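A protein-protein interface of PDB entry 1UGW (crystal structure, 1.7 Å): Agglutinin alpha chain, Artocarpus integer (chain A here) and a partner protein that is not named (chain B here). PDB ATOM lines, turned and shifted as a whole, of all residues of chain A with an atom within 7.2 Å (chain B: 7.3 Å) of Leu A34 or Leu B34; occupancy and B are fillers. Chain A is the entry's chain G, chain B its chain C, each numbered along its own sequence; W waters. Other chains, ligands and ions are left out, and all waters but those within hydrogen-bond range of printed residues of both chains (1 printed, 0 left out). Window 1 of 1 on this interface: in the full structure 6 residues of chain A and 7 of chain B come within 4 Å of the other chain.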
ATOM      1  N   ASP A   6      -4.231 -11.448  -4.796  1.00  0.00           N
ATOM      2  CA  ASP A   6      -3.580 -10.441  -3.963  1.00  0.00           C
ATOM      3  C   ASP A   6      -4.314 -10.195  -2.653  1.00  0.00           C
ATOM      4  O   ASP A   6      -3.699  -9.853  -1.646  1.00  0.00           O
ATOM      5  CB  ASP A   6      -3.470  -9.105  -4.701  1.00  0.00           C
ATOM      6  CG  ASP A   6      -2.476  -9.140  -5.844  1.00  0.00           C
ATOM      7  OD1 ASP A   6      -1.673 -10.096  -5.922  1.00  0.00           O
ATOM      8  OD2 ASP A   6      -2.494  -8.194  -6.654  1.00  0.00           O
ATOM      9  N   GLY A   7      -5.628 -10.365  -2.668  1.00  0.00           N
ATOM     10  CA  GLY A   7      -6.402 -10.117  -1.466  1.00  0.00           C
ATOM     11  C   GLY A   7      -6.933  -8.695  -1.492  1.00  0.00           C
ATOM     12  O   GLY A   7      -6.823  -8.005  -2.511  1.00  0.00           O
ATOM     13  N   ALA A   8      -7.495  -8.247  -0.373  1.00  0.00           N
ATOM     14  CA  ALA A   8      -8.061  -6.901  -0.289  1.00  0.00           C
ATOM     15  C   ALA A   8      -7.198  -5.942   0.522  1.00  0.00           C
ATOM     16  O   ALA A   8      -6.599  -6.329   1.529  1.00  0.00           O
ATOM     17  CB  ALA A   8      -9.462  -6.972   0.312  1.00  0.00           C
ATOM     18  N   PHE A   9      -7.150  -4.688   0.077  1.00  0.00           N
ATOM     19  CA  PHE A   9      -6.370  -3.648   0.736  1.00  0.00           C
ATOM     20  C   PHE A   9      -7.198  -2.387   1.003  1.00  0.00           C
ATOM     21  O   PHE A   9      -8.427  -2.422   0.951  1.00  0.00           O
ATOM     22  CB  PHE A   9      -5.129  -3.310  -0.103  1.00  0.00           C
ATOM     23  CG  PHE A   9      -4.157  -4.451  -0.215  1.00  0.00           C
ATOM     24  CD1 PHE A   9      -4.383  -5.491  -1.110  1.00  0.00           C
ATOM     25  CD2 PHE A   9      -3.056  -4.522   0.633  1.00  0.00           C
ATOM     26  CE1 PHE A   9      -3.529  -6.594  -1.156  1.00  0.00           C
ATOM     27  CE2 PHE A   9      -2.197  -5.619   0.596  1.00  0.00           C
ATOM     28  CZ  PHE A   9      -2.437  -6.658  -0.301  1.00  0.00           C
ATOM     29  N   THR A  10      -6.509  -1.284   1.298  1.00  0.00           N
ATOM     30  CA  THR A  10      -7.144  -0.004   1.611  1.00  0.00           C
ATOM     31  C   THR A  10      -7.433   0.834   0.374  1.00  0.00           C
ATOM     32  O   THR A  10      -8.268   1.738   0.413  1.00  0.00           O
ATOM     33  CB  THR A  10      -6.243   0.850   2.533  1.00  0.00           C
ATOM     34  OG1 THR A  10      -5.677   0.022   3.550  1.00  0.00           O
ATOM     35  CG2 THR A  10      -7.050   1.955   3.190  1.00  0.00           C
ATOM     36  N   GLY A  11      -6.724   0.541  -0.713  1.00  0.00           N
ATOM     37  CA  GLY A  11      -6.911   1.290  -1.938  1.00  0.00           C
ATOM     38  C   GLY A  11      -5.850   0.928  -2.957  1.00  0.00           C
ATOM     39  O   GLY A  11      -5.082  -0.019  -2.753  1.00  0.00           O
ATOM     40  N   ARG A  13      -2.696   2.495  -5.489  1.00  0.00           N
ATOM     41  CA  ARG A  13      -1.776   3.597  -5.767  1.00  0.00           C
ATOM     42  C   ARG A  13      -1.176   3.555  -7.169  1.00  0.00           C
ATOM     43  O   ARG A  13      -0.958   4.596  -7.786  1.00  0.00           O
ATOM     44  CB  ARG A  13      -0.632   3.609  -4.747  1.00  0.00           C
ATOM     45  CG  ARG A  13      -1.027   4.094  -3.357  1.00  0.00           C
ATOM     46  CD  ARG A  13       0.102   3.858  -2.360  1.00  0.00           C
ATOM     47  NE  ARG A  13      -0.212   4.406  -1.042  1.00  0.00           N
ATOM     48  CZ  ARG A  13       0.045   5.656  -0.663  1.00  0.00           C
ATOM     49  NH1 ARG A  13       0.634   6.508  -1.499  1.00  0.00           N
ATOM     50  NH2 ARG A  13      -0.299   6.059   0.552  1.00  0.00           N
ATOM     51  N   TYR A  32      -0.615  -1.392  -3.890  1.00  0.00           N
ATOM     52  CA  TYR A  32      -1.797  -1.032  -3.122  1.00  0.00           C
ATOM     53  C   TYR A  32      -1.485  -0.045  -2.020  1.00  0.00           C
ATOM     54  O   TYR A  32      -0.329   0.312  -1.782  1.00  0.00           O
ATOM     55  CB  TYR A  32      -2.390  -2.275  -2.453  1.00  0.00           C
ATOM     56  CG  TYR A  32      -2.863  -3.337  -3.402  1.00  0.00           C
ATOM     57  CD1 TYR A  32      -2.040  -4.408  -3.758  1.00  0.00           C
ATOM     58  CD2 TYR A  32      -4.137  -3.270  -3.956  1.00  0.00           C
ATOM     59  CE1 TYR A  32      -2.480  -5.387  -4.644  1.00  0.00           C
ATOM     60  CE2 TYR A  32      -4.584  -4.237  -4.841  1.00  0.00           C
ATOM     61  CZ  TYR A  32      -3.758  -5.289  -5.181  1.00  0.00           C
ATOM     62  OH  TYR A  32      -4.221  -6.231  -6.063  1.00  0.00           O
ATOM     63  N   ASP A  33      -2.537   0.412  -1.357  1.00  0.00           N
ATOM     64  CA  ASP A  33      -2.344   1.255  -0.197  1.00  0.00           C
ATOM     65  C   ASP A  33      -2.754   0.334   0.942  1.00  0.00           C
ATOM     66  O   ASP A  33      -3.731  -0.409   0.818  1.00  0.00           O
ATOM     67  CB  ASP A  33      -3.264   2.475  -0.176  1.00  0.00           C
ATOM     68  CG  ASP A  33      -3.076   3.302   1.087  1.00  0.00           C
ATOM     69  OD1 ASP A  33      -1.987   3.887   1.255  1.00  0.00           O
ATOM     70  OD2 ASP A  33      -3.999   3.348   1.929  1.00  0.00           O
ATOM     71  N   LEU A  34      -1.993   0.353   2.026  1.00  0.00           N
ATOM     72  CA  LEU A  34      -2.332  -0.444   3.195  1.00  0.00           C
ATOM     73  C   LEU A  34      -2.309   0.523   4.366  1.00  0.00           C
ATOM     74  O   LEU A  34      -1.251   0.823   4.916  1.00  0.00           O
ATOM     75  CB  LEU A  34      -1.321  -1.570   3.424  1.00  0.00           C
ATOM     76  CG  LEU A  34      -1.553  -2.426   4.679  1.00  0.00           C
ATOM     77  CD1 LEU A  34      -2.889  -3.148   4.575  1.00  0.00           C
ATOM     78  CD2 LEU A  34      -0.409  -3.426   4.841  1.00  0.00           C
ATOM     79  N   ASN A  35      -3.483   1.032   4.713  1.00  0.00           N
ATOM     80  CA  ASN A  35      -3.626   1.962   5.824  1.00  0.00           C
ATOM     81  C   ASN A  35      -2.649   3.141   5.741  1.00  0.00           C
ATOM     82  O   ASN A  35      -2.021   3.516   6.732  1.00  0.00           O
ATOM     83  CB  ASN A  35      -3.456   1.203   7.146  1.00  0.00           C
ATOM     84  CG  ASN A  35      -4.428   0.037   7.275  1.00  0.00           C
ATOM     85  OD1 ASN A  35      -4.029  -1.093   7.566  1.00  0.00           O
ATOM     86  ND2 ASN A  35      -5.706   0.307   7.052  1.00  0.00           N
ATOM     87  N   GLY A  36      -2.522   3.715   4.547  1.00  0.00           N
ATOM     88  CA  GLY A  36      -1.652   4.865   4.363  1.00  0.00           C
ATOM     89  C   GLY A  36      -0.227   4.593   3.924  1.00  0.00           C
ATOM     90  O   GLY A  36       0.533   5.527   3.668  1.00  0.00           O
ATOM     91  N   SER A  37       0.150   3.324   3.852  1.00  0.00           N
ATOM     92  CA  SER A  37       1.496   2.966   3.431  1.00  0.00           C
ATOM     93  C   SER A  37       1.428   2.154   2.148  1.00  0.00           C
ATOM     94  O   SER A  37       0.593   1.261   2.015  1.00  0.00           O
ATOM     95  CB  SER A  37       2.193   2.143   4.519  1.00  0.00           C
ATOM     96  OG  SER A  37       3.430   1.625   4.054  1.00  0.00           O
ATOM     97  N   PRO A  38       2.296   2.468   1.174  1.00  0.00           N
ATOM     98  CA  PRO A  38       2.278   1.716  -0.081  1.00  0.00           C
ATOM     99  C   PRO A  38       2.631   0.261   0.196  1.00  0.00           C
ATOM    100  O   PRO A  38       3.499  -0.027   1.025  1.00  0.00           O
ATOM    101  CB  PRO A  38       3.362   2.400  -0.913  1.00  0.00           C
ATOM    102  CG  PRO A  38       3.376   3.800  -0.378  1.00  0.00           C
ATOM    103  CD  PRO A  38       3.261   3.577   1.107  1.00  0.00           C
ATOM    104  N   TYR A  39       1.955  -0.655  -0.487  1.00  0.00           N
ATOM    105  CA  TYR A  39       2.244  -2.067  -0.323  1.00  0.00           C
ATOM    106  C   TYR A  39       2.409  -2.643  -1.720  1.00  0.00           C
ATOM    107  O   TYR A  39       1.467  -2.674  -2.504  1.00  0.00           O
ATOM    108  CB  TYR A  39       1.116  -2.768   0.443  1.00  0.00           C
ATOM    109  CG  TYR A  39       1.408  -4.225   0.712  1.00  0.00           C
ATOM    110  CD1 TYR A  39       1.183  -5.192  -0.267  1.00  0.00           C
ATOM    111  CD2 TYR A  39       1.964  -4.631   1.924  1.00  0.00           C
ATOM    112  CE1 TYR A  39       1.507  -6.526  -0.050  1.00  0.00           C
ATOM    113  CE2 TYR A  39       2.295  -5.968   2.151  1.00  0.00           C
ATOM    114  CZ  TYR A  39       2.065  -6.906   1.158  1.00  0.00           C
ATOM    115  OH  TYR A  39       2.401  -8.225   1.361  1.00  0.00           O
ATOM    116  N   PHE A  60      -3.146   9.129  -5.673  1.00  0.00           N
ATOM    117  CA  PHE A  60      -3.814   8.637  -4.467  1.00  0.00           C
ATOM    118  C   PHE A  60      -3.664   9.669  -3.351  1.00  0.00           C
ATOM    119  O   PHE A  60      -2.585  10.233  -3.168  1.00  0.00           O
ATOM    120  CB  PHE A  60      -3.171   7.311  -4.038  1.00  0.00           C
ATOM    121  CG  PHE A  60      -3.778   6.706  -2.803  1.00  0.00           C
ATOM    122  CD1 PHE A  60      -4.945   5.951  -2.881  1.00  0.00           C
ATOM    123  CD2 PHE A  60      -3.190   6.906  -1.557  1.00  0.00           C
ATOM    124  CE1 PHE A  60      -5.520   5.405  -1.735  1.00  0.00           C
ATOM    125  CE2 PHE A  60      -3.756   6.365  -0.403  1.00  0.00           C
ATOM    126  CZ  PHE A  60      -4.925   5.613  -0.494  1.00  0.00           C
ATOM    127  N   ASP B   6      -3.094   1.412  13.912  1.00  0.00           N
ATOM    128  CA  ASP B   6      -2.626   0.296  13.094  1.00  0.00           C
ATOM    129  C   ASP B   6      -3.382   0.177  11.784  1.00  0.00           C
ATOM    130  O   ASP B   6      -2.845  -0.325  10.799  1.00  0.00           O
ATOM    131  CB  ASP B   6      -2.758  -1.034  13.840  1.00  0.00           C
ATOM    132  CG  ASP B   6      -1.792  -1.160  14.998  1.00  0.00           C
ATOM    133  OD1 ASP B   6      -0.858  -0.336  15.101  1.00  0.00           O
ATOM    134  OD2 ASP B   6      -1.965  -2.101  15.795  1.00  0.00           O
ATOM    135  N   GLY B   7      -4.630   0.632  11.770  1.00  0.00           N
ATOM    136  CA  GLY B   7      -5.425   0.516  10.562  1.00  0.00           C
ATOM    137  C   GLY B   7      -6.212  -0.784  10.565  1.00  0.00           C
ATOM    138  O   GLY B   7      -6.245  -1.497  11.572  1.00  0.00           O
ATOM    139  N   ALA B   8      -6.825  -1.110   9.433  1.00  0.00           N
ATOM    140  CA  ALA B   8      -7.641  -2.313   9.316  1.00  0.00           C
ATOM    141  C   ALA B   8      -6.966  -3.436   8.535  1.00  0.00           C
ATOM    142  O   ALA B   8      -6.310  -3.198   7.519  1.00  0.00           O
ATOM    143  CB  ALA B   8      -8.977  -1.964   8.661  1.00  0.00           C
ATOM    144  N   PHE B   9      -7.155  -4.665   9.007  1.00  0.00           N
ATOM    145  CA  PHE B   9      -6.574  -5.834   8.366  1.00  0.00           C
ATOM    146  C   PHE B   9      -7.629  -6.909   8.109  1.00  0.00           C
ATOM    147  O   PHE B   9      -8.829  -6.623   8.143  1.00  0.00           O
ATOM    148  CB  PHE B   9      -5.428  -6.389   9.226  1.00  0.00           C
ATOM    149  CG  PHE B   9      -4.258  -5.455   9.336  1.00  0.00           C
ATOM    150  CD1 PHE B   9      -4.285  -4.379  10.224  1.00  0.00           C
ATOM    151  CD2 PHE B   9      -3.150  -5.611   8.511  1.00  0.00           C
ATOM    152  CE1 PHE B   9      -3.224  -3.472  10.283  1.00  0.00           C
ATOM    153  CE2 PHE B   9      -2.083  -4.706   8.562  1.00  0.00           C
ATOM    154  CZ  PHE B   9      -2.124  -3.636   9.450  1.00  0.00           C
ATOM    155  N   THR B  10      -7.177  -8.137   7.857  1.00  0.00           N
ATOM    156  CA  THR B  10      -8.066  -9.263   7.560  1.00  0.00           C
ATOM    157  C   THR B  10      -8.483 -10.046   8.799  1.00  0.00           C
ATOM    158  O   THR B  10      -9.480 -10.773   8.779  1.00  0.00           O
ATOM    159  CB  THR B  10      -7.388 -10.267   6.597  1.00  0.00           C
ATOM    160  OG1 THR B  10      -6.776  -9.559   5.518  1.00  0.00           O
ATOM    161  CG2 THR B  10      -8.417 -11.230   6.033  1.00  0.00           C
ATOM    162  N   GLY B  11      -7.709  -9.911   9.869  1.00  0.00           N
ATOM    163  CA  GLY B  11      -8.020 -10.627  11.092  1.00  0.00           C
ATOM    164  C   GLY B  11      -6.937 -10.431  12.132  1.00  0.00           C
ATOM    165  O   GLY B  11      -6.013  -9.639  11.930  1.00  0.00           O
ATOM    166  N   ARG B  13      -4.154 -12.479  14.738  1.00  0.00           N
ATOM    167  CA  ARG B  13      -3.460 -13.728  15.023  1.00  0.00           C
ATOM    168  C   ARG B  13      -2.879 -13.786  16.432  1.00  0.00           C
ATOM    169  O   ARG B  13      -2.901 -14.833  17.077  1.00  0.00           O
ATOM    170  CB  ARG B  13      -2.323 -13.949  14.013  1.00  0.00           C
ATOM    171  CG  ARG B  13      -2.793 -14.243  12.595  1.00  0.00           C
ATOM    172  CD  ARG B  13      -1.610 -14.357  11.636  1.00  0.00           C
ATOM    173  NE  ARG B  13      -2.012 -14.879  10.330  1.00  0.00           N
ATOM    174  CZ  ARG B  13      -1.981 -16.167   9.992  1.00  0.00           C
ATOM    175  NH1 ARG B  13      -2.370 -16.542   8.784  1.00  0.00           N
ATOM    176  NH2 ARG B  13      -1.542 -17.077  10.852  1.00  0.00           N
ATOM    177  N   TYR B  32      -1.336  -9.119  13.028  1.00  0.00           N
ATOM    178  CA  TYR B  32      -2.566  -9.241  12.259  1.00  0.00           C
ATOM    179  C   TYR B  32      -2.429 -10.273  11.160  1.00  0.00           C
ATOM    180  O   TYR B  32      -1.354 -10.815  10.928  1.00  0.00           O
ATOM    181  CB  TYR B  32      -2.910  -7.911  11.580  1.00  0.00           C
ATOM    182  CG  TYR B  32      -3.178  -6.773  12.520  1.00  0.00           C
ATOM    183  CD1 TYR B  32      -2.167  -5.876  12.874  1.00  0.00           C
ATOM    184  CD2 TYR B  32      -4.442  -6.601  13.079  1.00  0.00           C
ATOM    185  CE1 TYR B  32      -2.418  -4.828  13.768  1.00  0.00           C
ATOM    186  CE2 TYR B  32      -4.701  -5.570  13.964  1.00  0.00           C
ATOM    187  CZ  TYR B  32      -3.690  -4.686  14.307  1.00  0.00           C
ATOM    188  OH  TYR B  32      -3.966  -3.663  15.184  1.00  0.00           O
ATOM    189  N   ASP B  33      -3.542 -10.553  10.500  1.00  0.00           N
ATOM    190  CA  ASP B  33      -3.513 -11.429   9.345  1.00  0.00           C
ATOM    191  C   ASP B  33      -3.799 -10.465   8.211  1.00  0.00           C
ATOM    192  O   ASP B  33      -4.660  -9.590   8.346  1.00  0.00           O
ATOM    193  CB  ASP B  33      -4.625 -12.471   9.349  1.00  0.00           C
ATOM    194  CG  ASP B  33      -4.608 -13.316   8.090  1.00  0.00           C
ATOM    195  OD1 ASP B  33      -3.668 -14.121   7.942  1.00  0.00           O
ATOM    196  OD2 ASP B  33      -5.515 -13.159   7.239  1.00  0.00           O
ATOM    197  N   LEU B  34      -3.061 -10.601   7.117  1.00  0.00           N
ATOM    198  CA  LEU B  34      -3.269  -9.753   5.949  1.00  0.00           C
ATOM    199  C   LEU B  34      -3.428 -10.684   4.760  1.00  0.00           C
ATOM    200  O   LEU B  34      -2.443 -11.133   4.178  1.00  0.00           O
ATOM    201  CB  LEU B  34      -2.078  -8.825   5.711  1.00  0.00           C
ATOM    202  CG  LEU B  34      -2.197  -7.947   4.457  1.00  0.00           C
ATOM    203  CD1 LEU B  34      -3.422  -7.051   4.574  1.00  0.00           C
ATOM    204  CD2 LEU B  34      -0.931  -7.112   4.280  1.00  0.00           C
ATOM    205  N   ASN B  35      -4.677 -10.989   4.430  1.00  0.00           N
ATOM    206  CA  ASN B  35      -4.995 -11.860   3.307  1.00  0.00           C
ATOM    207  C   ASN B  35      -4.300 -13.217   3.391  1.00  0.00           C
ATOM    208  O   ASN B  35      -3.799 -13.729   2.392  1.00  0.00           O
ATOM    209  CB  ASN B  35      -4.635 -11.149   1.994  1.00  0.00           C
ATOM    210  CG  ASN B  35      -5.348  -9.815   1.847  1.00  0.00           C
ATOM    211  OD1 ASN B  35      -4.721  -8.778   1.607  1.00  0.00           O
ATOM    212  ND2 ASN B  35      -6.661  -9.835   1.991  1.00  0.00           N
ATOM    213  N   GLY B  36      -4.263 -13.791   4.593  1.00  0.00           N
ATOM    214  CA  GLY B  36      -3.650 -15.098   4.768  1.00  0.00           C
ATOM    215  C   GLY B  36      -2.208 -15.111   5.242  1.00  0.00           C
ATOM    216  O   GLY B  36      -1.671 -16.177   5.547  1.00  0.00           O
ATOM    217  N   SER B  37      -1.574 -13.944   5.301  1.00  0.00           N
ATOM    218  CA  SER B  37      -0.186 -13.859   5.748  1.00  0.00           C
ATOM    219  C   SER B  37      -0.063 -13.042   7.027  1.00  0.00           C
ATOM    220  O   SER B  37      -0.734 -12.020   7.191  1.00  0.00           O
ATOM    221  CB  SER B  37       0.687 -13.214   4.667  1.00  0.00           C
ATOM    222  OG  SER B  37       0.738 -14.016   3.499  1.00  0.00           O
ATOM    223  N   PRO B  38       0.792 -13.487   7.960  1.00  0.00           N
ATOM    224  CA  PRO B  38       0.957 -12.736   9.205  1.00  0.00           C
ATOM    225  C   PRO B  38       1.550 -11.374   8.870  1.00  0.00           C
ATOM    226  O   PRO B  38       2.371 -11.258   7.960  1.00  0.00           O
ATOM    227  CB  PRO B  38       1.947 -13.590  10.002  1.00  0.00           C
ATOM    228  CG  PRO B  38       1.715 -14.980   9.476  1.00  0.00           C
ATOM    229  CD  PRO B  38       1.559 -14.745   7.994  1.00  0.00           C
ATOM    230  N   TYR B  39       1.116 -10.346   9.589  1.00  0.00           N
ATOM    231  CA  TYR B  39       1.639  -8.999   9.396  1.00  0.00           C
ATOM    232  C   TYR B  39       1.841  -8.455  10.798  1.00  0.00           C
ATOM    233  O   TYR B  39       0.882  -8.282  11.553  1.00  0.00           O
ATOM    234  CB  TYR B  39       0.660  -8.120   8.612  1.00  0.00           C
ATOM    235  CG  TYR B  39       1.246  -6.771   8.240  1.00  0.00           C
ATOM    236  CD1 TYR B  39       1.277  -5.719   9.159  1.00  0.00           C
ATOM    237  CD2 TYR B  39       1.817  -6.564   6.983  1.00  0.00           C
ATOM    238  CE1 TYR B  39       1.864  -4.493   8.837  1.00  0.00           C
ATOM    239  CE2 TYR B  39       2.410  -5.342   6.650  1.00  0.00           C
ATOM    240  CZ  TYR B  39       2.429  -4.316   7.580  1.00  0.00           C
ATOM    241  OH  TYR B  39       3.024  -3.118   7.259  1.00  0.00           O
ATOM    242  N   PHE B  60      -5.867 -18.843  14.865  1.00  0.00           N
ATOM    243  CA  PHE B  60      -6.438 -18.252  13.659  1.00  0.00           C
ATOM    244  C   PHE B  60      -6.519 -19.315  12.557  1.00  0.00           C
ATOM    245  O   PHE B  60      -5.574 -20.074  12.358  1.00  0.00           O
ATOM    246  CB  PHE B  60      -5.548 -17.092  13.203  1.00  0.00           C
ATOM    247  CG  PHE B  60      -6.029 -16.405  11.963  1.00  0.00           C
ATOM    248  CD1 PHE B  60      -7.030 -15.441  12.028  1.00  0.00           C
ATOM    249  CD2 PHE B  60      -5.486 -16.730  10.721  1.00  0.00           C
ATOM    250  CE1 PHE B  60      -7.483 -14.807  10.875  1.00  0.00           C
ATOM    251  CE2 PHE B  60      -5.933 -16.102   9.562  1.00  0.00           C
ATOM    252  CZ  PHE B  60      -6.934 -15.139   9.639  1.00  0.00           C
HETATM  253  O   HOH W   1       4.266  -0.994   5.601  1.00  0.00           O
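The side-chain hydroxyl (OH) of Tyr A32 lies within hydrogen-bond range of the side-chain carboxylate (OD2) of Asp A6 (2.7 Å).
The backbone NH (N) of Asn A35 lies within hydrogen-bond range of the side-chain hydroxyl (OG1) of Thr A10 (2.7 Å).
OD2 of Asp B6 sits at hydrogen-bond distance from OH of Tyr B32, at 2.6 Å.
The side-chain hydroxyl (OG1) of Thr B10 sits at hydrogen-bond distance from the backbone NH (N) of Asn B35.
The backbone NH (N) of Tyr B32 sits at hydrogen-bond distance from the backbone carbonyl oxygen (O) of Tyr B39, 2.8 Å away.
Water W1 lies within hydrogen-bond range of OH of Tyr B39 (3.0 Å) and OG of Ser A37 (3.2 Å).
Of the printed residues of chain B, Ala A8 touches Asn B35 (3.0 Å).
Printed residues of chain B within 4 Å of Phe A9: Asn B35.
Of chain B, only Leu B34 (3.8 Å) and Tyr B39 (3.9 Å) come within 4 Å of Leu A34.
Printed residues of chain A within 4 Å of Gly B7: Asn A35 (3.5 Å).
Printed residues of chain A within 4 Å of Ala B8: Asn A35.
Thr B10 touches none of the printed residues of chain A.
Of the printed residues of chain A, Leu B34 touches Leu A34 (3.8 Å).
Of the printed residues of chain A, Tyr B39 touches Leu A34.
The nearest residue of chain B that does not touch Leu A34 is Phe B9 (4.3 Å).
The nearest residue of chain A that does not touch Leu B34 is Tyr A39 (4.03 Å).
The nearest printed residue of chain B that does not touch Ala A8 is Leu B34 (4.5 Å).
Among the printed residues, pairs that only touch across the chains: Asp A6 with Asn B35, Gly A7 with Asn B35, Phe A9 with Asn B35, Leu A34 with Leu B34, Leu A34 with Tyr B39, Asn A35 with Asp B6, Asn A35 with Gly B7 and Asn A35 with Phe B9.
N of Ala A8 lies close to ND2 of Asn B35, at 3.0 Å.
The side-chain amide nitrogen of Asn A35 lies close to the backbone NH of Ala B8 (3.0 Å).
Printed residues of chain B that touch a printed residue of chain A: Asp B6, Gly B7, Ala B8, Phe B9, Leu B34, Asn B35 and Tyr B39.
Hydrophobic or aromatic side chains of chain B within 4 Å of the printed part of chain A: Phe B9, Leu B34 and Tyr B39.
Of the 16 printed residues of chain A, 6 touch a printed residue of chain B.
Hydrophobic or aromatic side chains of chain A within 4 Å of the printed part of chain B: Phe A9 and Leu A34.
Among the printed residues, 10 pairs touch across the chains.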
